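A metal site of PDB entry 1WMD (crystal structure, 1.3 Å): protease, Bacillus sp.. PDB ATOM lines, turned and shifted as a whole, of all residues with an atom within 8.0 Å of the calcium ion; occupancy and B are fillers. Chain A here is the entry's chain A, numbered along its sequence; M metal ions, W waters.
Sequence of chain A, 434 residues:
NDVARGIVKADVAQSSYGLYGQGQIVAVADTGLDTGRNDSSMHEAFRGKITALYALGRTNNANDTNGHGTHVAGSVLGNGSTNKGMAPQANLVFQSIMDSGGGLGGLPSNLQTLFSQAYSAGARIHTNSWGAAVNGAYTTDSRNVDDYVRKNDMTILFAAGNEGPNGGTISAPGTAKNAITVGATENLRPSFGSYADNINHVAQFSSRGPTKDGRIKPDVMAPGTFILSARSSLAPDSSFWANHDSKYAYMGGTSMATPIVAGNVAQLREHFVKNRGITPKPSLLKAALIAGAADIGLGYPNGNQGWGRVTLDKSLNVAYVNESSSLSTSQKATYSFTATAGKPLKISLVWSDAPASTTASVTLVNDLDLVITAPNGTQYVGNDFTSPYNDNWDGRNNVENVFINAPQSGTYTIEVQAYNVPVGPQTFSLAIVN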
ATOM      1  N   GLU A 186      13.830  -6.594  18.348  1.00  0.00           N
ATOM      2  CA  GLU A 186      12.937  -7.706  18.000  1.00  0.00           C
ATOM      3  C   GLU A 186      13.014  -8.054  16.519  1.00  0.00           C
ATOM      4  O   GLU A 186      13.094  -7.175  15.654  1.00  0.00           O
ATOM      5  CB  GLU A 186      11.480  -7.347  18.358  1.00  0.00           C
ATOM      6  CG  GLU A 186      11.369  -7.179  19.896  1.00  0.00           C
ATOM      7  CD  GLU A 186       9.932  -6.915  20.326  1.00  0.00           C
ATOM      8  OE1 GLU A 186       9.732  -6.724  21.553  1.00  0.00           O
ATOM      9  OE2 GLU A 186       9.006  -6.766  19.485  1.00  0.00           O
ATOM     10  N   ASN A 187      12.929  -9.334  16.174  1.00  0.00           N
ATOM     11  CA  ASN A 187      12.626  -9.732  14.801  1.00  0.00           C
ATOM     12  C   ASN A 187      11.166  -9.450  14.485  1.00  0.00           C
ATOM     13  O   ASN A 187      10.355  -9.283  15.413  1.00  0.00           O
ATOM     14  CB  ASN A 187      12.926 -11.220  14.646  1.00  0.00           C
ATOM     15  CG  ASN A 187      13.293 -11.679  13.241  1.00  0.00           C
ATOM     16  OD1 ASN A 187      13.553 -10.827  12.370  1.00  0.00           O
ATOM     17  ND2 ASN A 187      13.418 -12.968  13.006  1.00  0.00           N
ATOM     18  N   GLY A 193       4.030 -13.393  18.766  1.00  0.00           N
ATOM     19  CA  GLY A 193       3.607 -12.549  19.885  1.00  0.00           C
ATOM     20  C   GLY A 193       4.525 -11.369  20.133  1.00  0.00           C
ATOM     21  O   GLY A 193       5.281 -10.933  19.242  1.00  0.00           O
ATOM     22  N   SER A 194       4.425 -10.835  21.358  1.00  0.00           N
ATOM     23  CA  SER A 194       4.990  -9.527  21.628  1.00  0.00           C
ATOM     24  C   SER A 194       6.502  -9.458  21.595  1.00  0.00           C
ATOM     25  O   SER A 194       7.057  -8.363  21.528  1.00  0.00           O
ATOM     26  CB  SER A 194       4.498  -8.961  22.982  1.00  0.00           C
ATOM     27  OG  SER A 194       4.946  -9.777  24.057  1.00  0.00           O
ATOM     28  N   TYR A 195       7.184 -10.621  21.600  1.00  0.00           N
ATOM     29  CA  TYR A 195       8.627 -10.558  21.545  1.00  0.00           C
ATOM     30  C   TYR A 195       9.106 -10.328  20.111  1.00  0.00           C
ATOM     31  O   TYR A 195      10.288 -10.090  19.975  1.00  0.00           O
ATOM     32  CB  TYR A 195       9.302 -11.851  21.996  1.00  0.00           C
ATOM     33  CG  TYR A 195       9.774 -12.040  23.401  1.00  0.00           C
ATOM     34  CD1 TYR A 195       9.497 -13.191  24.129  1.00  0.00           C
ATOM     35  CD2 TYR A 195      10.552 -11.092  24.061  1.00  0.00           C
ATOM     36  CE1 TYR A 195       9.930 -13.394  25.428  1.00  0.00           C
ATOM     37  CE2 TYR A 195      11.003 -11.253  25.352  1.00  0.00           C
ATOM     38  CZ  TYR A 195      10.680 -12.414  26.031  1.00  0.00           C
ATOM     39  OH  TYR A 195      11.144 -12.561  27.310  1.00  0.00           O
ATOM     40  N   ALA A 196       8.232 -10.441  19.114  1.00  0.00           N
ATOM     41  CA  ALA A 196       8.662 -10.312  17.730  1.00  0.00           C
ATOM     42  C   ALA A 196       7.678  -9.494  16.919  1.00  0.00           C
ATOM     43  O   ALA A 196       7.289  -9.893  15.803  1.00  0.00           O
ATOM     44  CB  ALA A 196       8.932 -11.641  17.033  1.00  0.00           C
ATOM     45  N   ASP A 197       7.258  -8.354  17.466  1.00  0.00           N
ATOM     46  CA  ASP A 197       6.258  -7.594  16.716  1.00  0.00           C
ATOM     47  C   ASP A 197       6.716  -6.188  16.336  1.00  0.00           C
ATOM     48  O   ASP A 197       5.976  -5.520  15.586  1.00  0.00           O
ATOM     49  CB  ASP A 197       4.957  -7.542  17.498  1.00  0.00           C
ATOM     50  CG  ASP A 197       5.017  -6.780  18.801  1.00  0.00           C
ATOM     51  OD1 ASP A 197       6.121  -6.383  19.223  1.00  0.00           O
ATOM     52  OD2 ASP A 197       3.955  -6.588  19.466  1.00  0.00           O
ATOM     53  N   ASN A 198       7.852  -5.681  16.738  1.00  0.00           N
ATOM     54  CA  ASN A 198       8.259  -4.308  16.380  1.00  0.00           C
ATOM     55  C   ASN A 198       9.773  -4.255  16.210  1.00  0.00           C
ATOM     56  O   ASN A 198      10.471  -4.444  17.206  1.00  0.00           O
ATOM     57  CB  ASN A 198       7.763  -3.297  17.437  1.00  0.00           C
ATOM     58  CG  ASN A 198       8.011  -1.883  16.969  1.00  0.00           C
ATOM     59  OD1 ASN A 198       8.919  -1.588  16.186  1.00  0.00           O
ATOM     60  ND2 ASN A 198       7.149  -0.924  17.396  1.00  0.00           N
ATOM     61  N   ILE A 199      10.229  -4.044  14.957  1.00  0.00           N
ATOM     62  CA  ILE A 199      11.680  -4.087  14.775  1.00  0.00           C
ATOM     63  C   ILE A 199      12.397  -2.912  15.429  1.00  0.00           C
ATOM     64  O   ILE A 199      13.644  -2.965  15.509  1.00  0.00           O
ATOM     65  CB  ILE A 199      12.009  -4.064  13.265  1.00  0.00           C
ATOM     66  CG1 ILE A 199      11.689  -2.750  12.600  1.00  0.00           C
ATOM     67  CG2 ILE A 199      11.313  -5.246  12.593  1.00  0.00           C
ATOM     68  CD1 ILE A 199      12.292  -2.667  11.199  1.00  0.00           C
ATOM     69  N   ASN A 200      11.637  -1.920  15.903  1.00  0.00           N
ATOM     70  CA  ASN A 200      12.169  -0.795  16.667  1.00  0.00           C
ATOM     71  C   ASN A 200      11.996  -0.907  18.169  1.00  0.00           C
ATOM     72  O   ASN A 200      12.201   0.091  18.899  1.00  0.00           O
ATOM     73  CB  ASN A 200      11.544   0.506  16.147  1.00  0.00           C
ATOM     74  CG  ASN A 200      12.079   0.899  14.798  1.00  0.00           C
ATOM     75  OD1 ASN A 200      13.291   0.982  14.594  1.00  0.00           O
ATOM     76  ND2 ASN A 200      11.150   1.134  13.853  1.00  0.00           N
ATOM     77  N   HIS A 201      11.686  -2.137  18.658  1.00  0.00           N
ATOM     78  CA  HIS A 201      11.616  -2.445  20.082  1.00  0.00           C
ATOM     79  C   HIS A 201      12.938  -3.062  20.552  1.00  0.00           C
ATOM     80  O   HIS A 201      13.337  -4.025  19.888  1.00  0.00           O
ATOM     81  CB  HIS A 201      10.498  -3.433  20.472  1.00  0.00           C
ATOM     82  CG  HIS A 201       9.088  -2.965  20.604  1.00  0.00           C
ATOM     83  ND1 HIS A 201       7.896  -3.664  20.904  1.00  0.00           N
ATOM     84  CD2 HIS A 201       8.730  -1.678  20.430  1.00  0.00           C
ATOM     85  CE1 HIS A 201       6.897  -2.783  20.917  1.00  0.00           C
ATOM     86  NE2 HIS A 201       7.374  -1.566  20.613  1.00  0.00           N
ATOM     87  N   VAL A 202      13.539  -2.581  21.643  1.00  0.00           N
ATOM     88  CA  VAL A 202      14.630  -3.345  22.266  1.00  0.00           C
ATOM     89  C   VAL A 202      14.007  -4.582  22.923  1.00  0.00           C
ATOM     90  O   VAL A 202      13.009  -4.432  23.645  1.00  0.00           O
ATOM     91  CB  VAL A 202      15.335  -2.518  23.347  1.00  0.00           C
ATOM     92  CG1 VAL A 202      16.473  -3.344  23.938  1.00  0.00           C
ATOM     93  CG2 VAL A 202      15.826  -1.213  22.746  1.00  0.00           C
ATOM     94  N   ALA A 203      14.569  -5.765  22.678  1.00  0.00           N
ATOM     95  CA  ALA A 203      14.017  -6.953  23.329  1.00  0.00           C
ATOM     96  C   ALA A 203      14.080  -6.765  24.858  1.00  0.00           C
ATOM     97  O   ALA A 203      15.065  -6.225  25.375  1.00  0.00           O
ATOM     98  CB  ALA A 203      14.822  -8.177  22.923  1.00  0.00           C
ATOM     99  N   GLN A 204      13.050  -7.189  25.565  1.00  0.00           N
ATOM    100  CA  GLN A 204      12.970  -6.892  26.986  1.00  0.00           C
ATOM    101  C   GLN A 204      14.209  -7.296  27.777  1.00  0.00           C
ATOM    102  O   GLN A 204      14.681  -6.554  28.648  1.00  0.00           O
ATOM    103  CB  GLN A 204      11.722  -7.568  27.579  1.00  0.00           C
ATOM    104  CG  GLN A 204      11.527  -7.066  29.009  1.00  0.00           C
ATOM    105  CD  GLN A 204      10.203  -7.589  29.520  1.00  0.00           C
ATOM    106  OE1 GLN A 204      10.076  -8.813  29.548  1.00  0.00           O
ATOM    107  NE2 GLN A 204       9.283  -6.718  29.881  1.00  0.00           N
ATOM    108  N   THR A 225      15.189 -11.847  18.541  1.00  0.00           N
ATOM    109  CA  THR A 225      14.075 -12.666  19.056  1.00  0.00           C
ATOM    110  C   THR A 225      13.523 -13.571  17.959  1.00  0.00           C
ATOM    111  O   THR A 225      13.530 -13.150  16.819  1.00  0.00           O
ATOM    112  CB  THR A 225      12.949 -11.791  19.649  1.00  0.00           C
ATOM    113  OG1 THR A 225      12.364 -11.019  18.600  1.00  0.00           O
ATOM    114  CG2 THR A 225      13.459 -10.869  20.724  1.00  0.00           C
HETATM  115 CA    CA M   1       7.391  -6.148  21.213  1.00  0.00          CA
HETATM  116  O   HOH W   1       7.516  -5.734  23.531  1.00  0.00           O
HETATM  117  O   HOH W   2       5.129  -5.537  21.725  1.00  0.00           O
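Of the 15 residues printed, 4 come within 4 Å of the calcium ion.
Along chain A the residues within 4 Å of the calcium ion span positions 186 to 201.
The nearest printed residue that does not touch the calcium ion is Tyr 195 (4.5 Å).
NE2 of His 201 lies within hydrogen-bond range of ND2 of Asn 198, at 3.3 Å.
The backbone NH (N) of Asn 198 sits close to the side-chain carboxylate (OE2) of Glu 186 (3.2 Å).
The calcium ion is bound by O of Ser 194, water W1, OD1 of Asp 197, water W2, OE1 of Glu 186, OE2 of Glu 186 and ND1 of His 201.
The calcium ion has seven donor atoms within binding distance.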
